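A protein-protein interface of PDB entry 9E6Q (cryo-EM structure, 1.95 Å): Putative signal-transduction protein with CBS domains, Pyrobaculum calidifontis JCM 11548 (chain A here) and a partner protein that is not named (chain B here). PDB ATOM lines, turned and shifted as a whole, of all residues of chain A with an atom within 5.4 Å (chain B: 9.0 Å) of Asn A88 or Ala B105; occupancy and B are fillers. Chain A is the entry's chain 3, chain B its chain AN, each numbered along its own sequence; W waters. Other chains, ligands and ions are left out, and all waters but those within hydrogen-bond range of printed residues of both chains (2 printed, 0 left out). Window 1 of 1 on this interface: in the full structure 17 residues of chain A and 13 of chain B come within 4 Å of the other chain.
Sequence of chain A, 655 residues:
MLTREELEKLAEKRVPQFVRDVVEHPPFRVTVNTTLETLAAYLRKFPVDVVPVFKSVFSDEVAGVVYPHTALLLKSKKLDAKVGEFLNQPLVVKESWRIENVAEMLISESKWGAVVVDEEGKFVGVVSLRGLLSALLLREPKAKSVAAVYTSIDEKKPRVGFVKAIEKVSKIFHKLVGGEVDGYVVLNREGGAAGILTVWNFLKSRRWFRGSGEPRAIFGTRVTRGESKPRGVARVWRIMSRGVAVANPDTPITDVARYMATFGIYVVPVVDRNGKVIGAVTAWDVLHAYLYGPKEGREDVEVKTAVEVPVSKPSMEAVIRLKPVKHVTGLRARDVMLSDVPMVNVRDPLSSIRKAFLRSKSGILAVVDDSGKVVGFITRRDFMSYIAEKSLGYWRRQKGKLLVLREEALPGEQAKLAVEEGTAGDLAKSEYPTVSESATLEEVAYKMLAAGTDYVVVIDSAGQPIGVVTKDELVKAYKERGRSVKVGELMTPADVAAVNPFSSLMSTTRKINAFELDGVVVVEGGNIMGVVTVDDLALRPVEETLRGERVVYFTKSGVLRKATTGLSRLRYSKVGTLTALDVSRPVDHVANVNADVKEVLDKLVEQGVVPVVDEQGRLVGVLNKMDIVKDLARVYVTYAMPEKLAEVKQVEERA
The side-chain carboxylate (OE1) of Glu B100 lies within salt-bridge range of the guanidinium group (NE) of Arg B102 (2.8 Å). The backbone NH (N) of Glu B100 sits at hydrogen-bond distance from the backbone carbonyl oxygen (O) of Ser B122, 3.0 Å away. NE of Arg B111 sits at hydrogen-bond distance from O of Arg B102 (3.1 Å). The backbone carbonyl oxygen (O) of Val A65 is in hydrogen-bond range of the backbone NH (N) of Asn A88, 2.9 Å away. The backbone NH of Tyr A67 is in hydrogen-bond range of the side-chain hydroxyl of Thr A70 (3.2 Å).
The side-chain carboxylate (OE2) of Glu B100 sits at hydrogen-bond distance from the side-chain amide nitrogen (NE2) of Gln A89 (2.8 Å). The backbone carbonyl oxygen of Leu A87 is in hydrogen-bond range of the guanidinium group of Arg B102, at 3.0 Å. The side-chain amide nitrogen of Asn A88 sits at hydrogen-bond distance from the backbone carbonyl oxygen of Ala B105. The backbone NH (N) of Met B106 sits at hydrogen-bond distance from the backbone carbonyl oxygen (O) of Val A177 (2.9 Å). N of Ala B107 is in hydrogen-bond range of O of Gly A178 (3.2 Å). The backbone carbonyl oxygen of Gly A178 is in hydrogen-bond range of the backbone NH of Gly B108.
Water W2 lies within hydrogen-bond range of OD1 of Asn A88, OG1 of Thr A70, O of Phe A86 and N of Ala B105. Water W1 lies within hydrogen-bond range of the backbone carbonyl oxygen (O) of Gly A178 (2.9 Å) and the backbone NH (N) of Gly B108 (3.3 Å).
Among the printed residues, merely in contact across the chains: Leu A87 with Leu B104 (3.2 Å), His A69 with Met B106 (3.4 Å), Tyr A67 with Met B106 (3.5 Å), His A69 with Ala B105 (3.5 Å), Thr A70 with Ala B105 (3.6 Å), Phe A86 with Met B103 (3.6 Å), Gly A178 with Met B106 (3.6 Å), Leu A73 with Leu B112 (3.6 Å), Phe A86 with Leu B104 (3.7 Å), Val A177 with Ala B105 (3.8 Å), Gln A89 with Ala B124 (3.8 Å), Gly A178 with Leu B112 (3.8 Å), Leu A73 with Ala B105 (3.9 Å), Gln A89 with Arg B102 (3.9 Å) and Leu A73 with Met B103 (3.95 Å).
Hydrophobic or aromatic side chains of chain A within 4 Å of the printed part of chain B: Tyr A67, His A69, Leu A73 and Phe A86. Of the 15 printed residues of chain B, 10 touch a printed residue of chain A. Among the printed residues, 21 pairs touch across the chains.
Val A66 touches none of the printed residues of chain B. Of the printed residues of chain B, Tyr A67 touches Met B106. Of the printed residues of chain B, Leu A87 touches Arg B102 (3.0 Å) and Leu B104 (3.2 Å). Of the printed residues of chain A, Glu B100 touches Gln A89. Of chain A, only His A69 (3.5 Å), Thr A70 (3.6 Å), Leu A73 (3.9 Å), Asn A88 (2.9 Å) and Val A177 (3.8 Å) come within 4 Å of Ala B105. Of the printed residues of chain A, Ala B107 touches Gly A178 (3.2 Å). The nearest residue of chain B that does not touch Asn A88 is Leu B104 (4.04 Å). The nearest residue of chain A that does not touch Ala B105 is Tyr A67 (4.4 Å).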
ATOM      1  N   GLY A  64      10.939 -13.370   6.187  1.00  0.00           N
ATOM      2  CA  GLY A  64      10.071 -14.506   6.422  1.00  0.00           C
ATOM      3  C   GLY A  64       9.042 -14.602   5.313  1.00  0.00           C
ATOM      4  O   GLY A  64       9.185 -13.978   4.267  1.00  0.00           O
ATOM      5  N   VAL A  65       8.012 -15.403   5.568  1.00  0.00           N
ATOM      6  CA  VAL A  65       6.904 -15.546   4.638  1.00  0.00           C
ATOM      7  C   VAL A  65       5.596 -15.440   5.399  1.00  0.00           C
ATOM      8  O   VAL A  65       5.536 -15.624   6.615  1.00  0.00           O
ATOM      9  CB  VAL A  65       6.936 -16.873   3.854  1.00  0.00           C
ATOM     10  CG1 VAL A  65       8.170 -16.955   3.014  1.00  0.00           C
ATOM     11  CG2 VAL A  65       6.852 -18.049   4.796  1.00  0.00           C
ATOM     12  N   VAL A  66       4.538 -15.132   4.656  1.00  0.00           N
ATOM     13  CA  VAL A  66       3.175 -15.238   5.147  1.00  0.00           C
ATOM     14  C   VAL A  66       2.352 -15.922   4.069  1.00  0.00           C
ATOM     15  O   VAL A  66       2.732 -15.966   2.900  1.00  0.00           O
ATOM     16  CB  VAL A  66       2.554 -13.874   5.520  1.00  0.00           C
ATOM     17  CG1 VAL A  66       3.190 -13.335   6.777  1.00  0.00           C
ATOM     18  CG2 VAL A  66       2.687 -12.887   4.381  1.00  0.00           C
ATOM     19  N   TYR A  67       1.222 -16.460   4.475  1.00  0.00           N
ATOM     20  CA  TYR A  67       0.303 -17.159   3.604  1.00  0.00           C
ATOM     21  C   TYR A  67      -0.965 -16.345   3.431  1.00  0.00           C
ATOM     22  O   TYR A  67      -1.183 -15.360   4.142  1.00  0.00           O
ATOM     23  CB  TYR A  67      -0.001 -18.542   4.189  1.00  0.00           C
ATOM     24  CG  TYR A  67       1.236 -19.389   4.304  1.00  0.00           C
ATOM     25  CD1 TYR A  67       1.879 -19.863   3.170  1.00  0.00           C
ATOM     26  CD2 TYR A  67       1.786 -19.684   5.537  1.00  0.00           C
ATOM     27  CE1 TYR A  67       3.012 -20.621   3.262  1.00  0.00           C
ATOM     28  CE2 TYR A  67       2.920 -20.440   5.638  1.00  0.00           C
ATOM     29  CZ  TYR A  67       3.531 -20.906   4.497  1.00  0.00           C
ATOM     30  OH  TYR A  67       4.668 -21.662   4.599  1.00  0.00           O
ATOM     31  N   HIS A  69      -3.729 -17.098   4.404  1.00  0.00           N
ATOM     32  CA  HIS A  69      -4.409 -17.242   5.682  1.00  0.00           C
ATOM     33  C   HIS A  69      -4.016 -16.148   6.664  1.00  0.00           C
ATOM     34  O   HIS A  69      -4.812 -15.782   7.531  1.00  0.00           O
ATOM     35  CB  HIS A  69      -4.101 -18.619   6.267  1.00  0.00           C
ATOM     36  CG  HIS A  69      -4.221 -19.740   5.282  1.00  0.00           C
ATOM     37  ND1 HIS A  69      -3.505 -19.787   4.107  1.00  0.00           N
ATOM     38  CD2 HIS A  69      -4.972 -20.865   5.306  1.00  0.00           C
ATOM     39  CE1 HIS A  69      -3.817 -20.884   3.446  1.00  0.00           C
ATOM     40  NE2 HIS A  69      -4.703 -21.558   4.154  1.00  0.00           N
ATOM     41  N   THR A  70      -2.804 -15.606   6.539  1.00  0.00           N
ATOM     42  CA  THR A  70      -2.344 -14.581   7.470  1.00  0.00           C
ATOM     43  C   THR A  70      -3.189 -13.323   7.386  1.00  0.00           C
ATOM     44  O   THR A  70      -3.416 -12.662   8.402  1.00  0.00           O
ATOM     45  CB  THR A  70      -0.873 -14.266   7.209  1.00  0.00           C
ATOM     46  OG1 THR A  70      -0.137 -15.488   7.153  1.00  0.00           O
ATOM     47  CG2 THR A  70      -0.300 -13.395   8.300  1.00  0.00           C
ATOM     48  N   LEU A  73      -6.083 -13.037   9.871  1.00  0.00           N
ATOM     49  CA  LEU A  73      -5.861 -12.852  11.296  1.00  0.00           C
ATOM     50  C   LEU A  73      -6.318 -11.488  11.789  1.00  0.00           C
ATOM     51  O   LEU A  73      -6.226 -11.224  12.989  1.00  0.00           O
ATOM     52  CB  LEU A  73      -4.384 -13.046  11.626  1.00  0.00           C
ATOM     53  CG  LEU A  73      -3.831 -14.455  11.420  1.00  0.00           C
ATOM     54  CD1 LEU A  73      -2.366 -14.492  11.765  1.00  0.00           C
ATOM     55  CD2 LEU A  73      -4.597 -15.457  12.245  1.00  0.00           C
ATOM     56  N   PHE A  86       3.362 -11.527  12.251  1.00  0.00           N
ATOM     57  CA  PHE A  86       2.801 -12.856  12.037  1.00  0.00           C
ATOM     58  C   PHE A  86       3.602 -13.623  10.999  1.00  0.00           C
ATOM     59  O   PHE A  86       3.042 -14.305  10.139  1.00  0.00           O
ATOM     60  CB  PHE A  86       1.337 -12.774  11.612  1.00  0.00           C
ATOM     61  CG  PHE A  86       0.506 -11.871  12.461  1.00  0.00           C
ATOM     62  CD1 PHE A  86      -0.080 -12.340  13.618  1.00  0.00           C
ATOM     63  CD2 PHE A  86       0.307 -10.555  12.105  1.00  0.00           C
ATOM     64  CE1 PHE A  86      -0.843 -11.512  14.397  1.00  0.00           C
ATOM     65  CE2 PHE A  86      -0.451  -9.724  12.881  1.00  0.00           C
ATOM     66  CZ  PHE A  86      -1.029 -10.201  14.027  1.00  0.00           C
ATOM     67  N   LEU A  87       4.922 -13.544  11.077  1.00  0.00           N
ATOM     68  CA  LEU A  87       5.779 -14.191  10.095  1.00  0.00           C
ATOM     69  C   LEU A  87       5.911 -15.678  10.388  1.00  0.00           C
ATOM     70  O   LEU A  87       6.225 -16.072  11.512  1.00  0.00           O
ATOM     71  CB  LEU A  87       7.155 -13.534  10.092  1.00  0.00           C
ATOM     72  CG  LEU A  87       7.218 -12.092   9.597  1.00  0.00           C
ATOM     73  CD1 LEU A  87       8.651 -11.633   9.480  1.00  0.00           C
ATOM     74  CD2 LEU A  87       6.514 -11.954   8.269  1.00  0.00           C
ATOM     75  N   ASN A  88       5.673 -16.500   9.375  1.00  0.00           N
ATOM     76  CA  ASN A  88       5.926 -17.928   9.464  1.00  0.00           C
ATOM     77  C   ASN A  88       7.386 -18.218   9.156  1.00  0.00           C
ATOM     78  O   ASN A  88       8.057 -17.450   8.468  1.00  0.00           O
ATOM     79  CB  ASN A  88       5.045 -18.708   8.489  1.00  0.00           C
ATOM     80  CG  ASN A  88       3.574 -18.513   8.744  1.00  0.00           C
ATOM     81  OD1 ASN A  88       2.995 -17.516   8.333  1.00  0.00           O
ATOM     82  ND2 ASN A  88       2.957 -19.469   9.407  1.00  0.00           N
ATOM     83  N   GLN A  89       7.872 -19.335   9.673  1.00  0.00           N
ATOM     84  CA  GLN A  89       9.179 -19.829   9.261  1.00  0.00           C
ATOM     85  C   GLN A  89       9.053 -20.406   7.862  1.00  0.00           C
ATOM     86  O   GLN A  89       8.248 -21.320   7.652  1.00  0.00           O
ATOM     87  CB  GLN A  89       9.704 -20.889  10.222  1.00  0.00           C
ATOM     88  CG  GLN A  89       9.583 -20.520  11.680  1.00  0.00           C
ATOM     89  CD  GLN A  89      10.786 -19.761  12.179  1.00  0.00           C
ATOM     90  OE1 GLN A  89      11.803 -19.673  11.497  1.00  0.00           O
ATOM     91  NE2 GLN A  89      10.672 -19.189  13.367  1.00  0.00           N
ATOM     92  N   PRO A  90       9.794 -19.910   6.887  1.00  0.00           N
ATOM     93  CA  PRO A  90       9.647 -20.416   5.522  1.00  0.00           C
ATOM     94  C   PRO A  90      10.262 -21.791   5.337  1.00  0.00           C
ATOM     95  O   PRO A  90      11.249 -22.157   5.976  1.00  0.00           O
ATOM     96  CB  PRO A  90      10.385 -19.369   4.685  1.00  0.00           C
ATOM     97  CG  PRO A  90      11.387 -18.809   5.603  1.00  0.00           C
ATOM     98  CD  PRO A  90      10.780 -18.824   6.973  1.00  0.00           C
ATOM     99  N   VAL A 177      -8.328 -21.030   8.534  1.00  0.00           N
ATOM    100  CA  VAL A 177      -7.217 -20.115   8.782  1.00  0.00           C
ATOM    101  C   VAL A 177      -6.020 -20.865   9.342  1.00  0.00           C
ATOM    102  O   VAL A 177      -4.869 -20.575   8.998  1.00  0.00           O
ATOM    103  CB  VAL A 177      -7.663 -18.974   9.715  1.00  0.00           C
ATOM    104  CG1 VAL A 177      -6.493 -18.096  10.093  1.00  0.00           C
ATOM    105  CG2 VAL A 177      -8.736 -18.151   9.054  1.00  0.00           C
ATOM    106  N   GLY A 178      -6.268 -21.846  10.203  1.00  0.00           N
ATOM    107  CA  GLY A 178      -5.197 -22.662  10.728  1.00  0.00           C
ATOM    108  C   GLY A 178      -4.635 -23.670   9.760  1.00  0.00           C
ATOM    109  O   GLY A 178      -3.611 -24.284  10.055  1.00  0.00           O
ATOM    110  N   ALA B   3      13.868 -14.613  13.386  1.00  0.00           N
ATOM    111  CA  ALA B   3      14.529 -15.308  14.480  1.00  0.00           C
ATOM    112  C   ALA B   3      14.682 -14.418  15.704  1.00  0.00           C
ATOM    113  O   ALA B   3      15.004 -13.241  15.603  1.00  0.00           O
ATOM    114  CB  ALA B   3      15.877 -15.824  14.040  1.00  0.00           C
ATOM    115  N   GLU B 100       8.539 -22.275  19.592  1.00  0.00           N
ATOM    116  CA  GLU B 100       8.128 -20.902  19.852  1.00  0.00           C
ATOM    117  C   GLU B 100       6.609 -20.811  19.919  1.00  0.00           C
ATOM    118  O   GLU B 100       5.902 -21.449  19.139  1.00  0.00           O
ATOM    119  CB  GLU B 100       8.675 -19.946  18.785  1.00  0.00           C
ATOM    120  CG  GLU B 100       8.022 -20.069  17.424  1.00  0.00           C
ATOM    121  CD  GLU B 100       8.695 -19.220  16.367  1.00  0.00           C
ATOM    122  OE1 GLU B 100       9.326 -18.205  16.723  1.00  0.00           O
ATOM    123  OE2 GLU B 100       8.584 -19.559  15.173  1.00  0.00           O
ATOM    124  N   ARG B 102       3.940 -18.446  19.257  1.00  0.00           N
ATOM    125  CA  ARG B 102       3.553 -17.219  18.578  1.00  0.00           C
ATOM    126  C   ARG B 102       2.258 -17.443  17.815  1.00  0.00           C
ATOM    127  O   ARG B 102       1.993 -18.538  17.324  1.00  0.00           O
ATOM    128  CB  ARG B 102       4.636 -16.747  17.609  1.00  0.00           C
ATOM    129  CG  ARG B 102       5.899 -16.258  18.270  1.00  0.00           C
ATOM    130  CD  ARG B 102       6.766 -15.479  17.299  1.00  0.00           C
ATOM    131  NE  ARG B 102       7.277 -16.311  16.218  1.00  0.00           N
ATOM    132  CZ  ARG B 102       7.009 -16.123  14.933  1.00  0.00           C
ATOM    133  NH1 ARG B 102       6.236 -15.133  14.526  1.00  0.00           N
ATOM    134  NH2 ARG B 102       7.533 -16.948  14.034  1.00  0.00           N
ATOM    135  N   MET B 103       1.455 -16.393  17.707  1.00  0.00           N
ATOM    136  CA  MET B 103       0.220 -16.495  16.944  1.00  0.00           C
ATOM    137  C   MET B 103       0.530 -16.465  15.453  1.00  0.00           C
ATOM    138  O   MET B 103       1.222 -15.566  14.972  1.00  0.00           O
ATOM    139  CB  MET B 103      -0.732 -15.364  17.323  1.00  0.00           C
ATOM    140  CG  MET B 103      -2.186 -15.783  17.387  1.00  0.00           C
ATOM    141  SD  MET B 103      -3.093 -15.361  15.900  1.00  0.00           S
ATOM    142  CE  MET B 103      -3.212 -13.593  16.087  1.00  0.00           C
ATOM    143  N   LEU B 104       0.029 -17.455  14.723  1.00  0.00           N
ATOM    144  CA  LEU B 104       0.395 -17.616  13.325  1.00  0.00           C
ATOM    145  C   LEU B 104      -0.779 -18.166  12.537  1.00  0.00           C
ATOM    146  O   LEU B 104      -1.605 -18.904  13.071  1.00  0.00           O
ATOM    147  CB  LEU B 104       1.575 -18.573  13.163  1.00  0.00           C
ATOM    148  CG  LEU B 104       2.957 -18.119  13.594  1.00  0.00           C
ATOM    149  CD1 LEU B 104       3.894 -19.296  13.548  1.00  0.00           C
ATOM    150  CD2 LEU B 104       3.428 -17.015  12.691  1.00  0.00           C
ATOM    151  N   ALA B 105      -0.762 -17.968  11.218  1.00  0.00           N
ATOM    152  CA  ALA B 105      -1.792 -18.630  10.383  1.00  0.00           C
ATOM    153  C   ALA B 105      -1.139 -19.824   9.672  1.00  0.00           C
ATOM    154  O   ALA B 105       0.099 -19.879   9.639  1.00  0.00           O
ATOM    155  CB  ALA B 105      -2.412 -17.661   9.409  1.00  0.00           C
ATOM    156  N   MET B 106      -1.946 -20.752   9.152  1.00  0.00           N
ATOM    157  CA  MET B 106      -1.424 -21.940   8.422  1.00  0.00           C
ATOM    158  C   MET B 106      -0.439 -22.716   9.302  1.00  0.00           C
ATOM    159  O   MET B 106       0.606 -23.130   8.780  1.00  0.00           O
ATOM    160  CB  MET B 106      -0.762 -21.523   7.104  1.00  0.00           C
ATOM    161  CG  MET B 106      -1.581 -21.894   5.883  1.00  0.00           C
ATOM    162  SD  MET B 106      -0.585 -22.508   4.498  1.00  0.00           S
ATOM    163  CE  MET B 106      -1.437 -24.046   4.150  1.00  0.00           C
ATOM    164  N   ALA B 107      -0.746 -22.878  10.590  1.00  0.00           N
ATOM    165  CA  ALA B 107       0.085 -23.693  11.464  1.00  0.00           C
ATOM    166  C   ALA B 107      -0.746 -24.469  12.484  1.00  0.00           C
ATOM    167  O   ALA B 107      -0.208 -24.893  13.509  1.00  0.00           O
ATOM    168  CB  ALA B 107       1.110 -22.828  12.192  1.00  0.00           C
ATOM    169  N   GLY B 108      -2.035 -24.639  12.256  1.00  0.00           N
ATOM    170  CA  GLY B 108      -2.881 -25.334  13.203  1.00  0.00           C
ATOM    171  C   GLY B 108      -3.837 -24.395  13.911  1.00  0.00           C
ATOM    172  O   GLY B 108      -3.546 -23.218  14.136  1.00  0.00           O
ATOM    173  N   ALA B 109      -5.003 -24.927  14.274  1.00  0.00           N
ATOM    174  CA  ALA B 109      -6.039 -24.094  14.876  1.00  0.00           C
ATOM    175  C   ALA B 109      -5.638 -23.606  16.263  1.00  0.00           C
ATOM    176  O   ALA B 109      -5.965 -22.480  16.646  1.00  0.00           O
ATOM    177  CB  ALA B 109      -7.360 -24.856  14.936  1.00  0.00           C
ATOM    178  N   ARG B 111      -2.816 -22.677  17.278  1.00  0.00           N
ATOM    179  CA  ARG B 111      -1.913 -21.541  17.178  1.00  0.00           C
ATOM    180  C   ARG B 111      -2.655 -20.219  17.053  1.00  0.00           C
ATOM    181  O   ARG B 111      -2.023 -19.166  17.133  1.00  0.00           O
ATOM    182  CB  ARG B 111      -0.976 -21.741  15.991  1.00  0.00           C
ATOM    183  CG  ARG B 111       0.348 -21.046  16.120  1.00  0.00           C
ATOM    184  CD  ARG B 111       1.357 -21.902  16.849  1.00  0.00           C
ATOM    185  NE  ARG B 111       1.492 -21.499  18.242  1.00  0.00           N
ATOM    186  CZ  ARG B 111       1.655 -22.340  19.250  1.00  0.00           C
ATOM    187  NH1 ARG B 111       1.728 -23.642  19.056  1.00  0.00           N
ATOM    188  NH2 ARG B 111       1.747 -21.861  20.484  1.00  0.00           N
ATOM    189  N   LEU B 112      -3.966 -20.245  16.846  1.00  0.00           N
ATOM    190  CA  LEU B 112      -4.753 -19.030  16.736  1.00  0.00           C
ATOM    191  C   LEU B 112      -5.252 -18.514  18.077  1.00  0.00           C
ATOM    192  O   LEU B 112      -5.833 -17.428  18.123  1.00  0.00           O
ATOM    193  CB  LEU B 112      -5.938 -19.263  15.801  1.00  0.00           C
ATOM    194  CG  LEU B 112      -5.539 -19.807  14.429  1.00  0.00           C
ATOM    195  CD1 LEU B 112      -6.757 -20.200  13.639  1.00  0.00           C
ATOM    196  CD2 LEU B 112      -4.720 -18.796  13.665  1.00  0.00           C
ATOM    197  N   SER B 122       5.266 -24.305  18.263  1.00  0.00           N
ATOM    198  CA  SER B 122       5.576 -24.920  16.985  1.00  0.00           C
ATOM    199  C   SER B 122       7.076 -24.873  16.746  1.00  0.00           C
ATOM    200  O   SER B 122       7.774 -24.040  17.321  1.00  0.00           O
ATOM    201  CB  SER B 122       4.832 -24.201  15.866  1.00  0.00           C
ATOM    202  OG  SER B 122       5.126 -22.822  15.860  1.00  0.00           O
ATOM    203  N   PRO B 123       7.611 -25.768  15.914  1.00  0.00           N
ATOM    204  CA  PRO B 123       9.063 -25.793  15.701  1.00  0.00           C
ATOM    205  C   PRO B 123       9.576 -24.476  15.144  1.00  0.00           C
ATOM    206  O   PRO B 123       8.970 -23.872  14.260  1.00  0.00           O
ATOM    207  CB  PRO B 123       9.258 -26.939  14.706  1.00  0.00           C
ATOM    208  CG  PRO B 123       8.060 -27.764  14.829  1.00  0.00           C
ATOM    209  CD  PRO B 123       6.936 -26.879  15.228  1.00  0.00           C
ATOM    210  N   ALA B 124      10.713 -24.038  15.665  1.00  0.00           N
ATOM    211  CA  ALA B 124      11.289 -22.762  15.288  1.00  0.00           C
ATOM    212  C   ALA B 124      12.726 -22.855  14.811  1.00  0.00           C
ATOM    213  O   ALA B 124      13.261 -21.850  14.340  1.00  0.00           O
ATOM    214  CB  ALA B 124      11.222 -21.778  16.464  1.00  0.00           C
HETATM  215  O   HOH W   1      -1.624 -26.311   9.409  1.00  0.00           O
HETATM  216  O   HOH W   2       1.065 -16.186   9.506  1.00  0.00           O
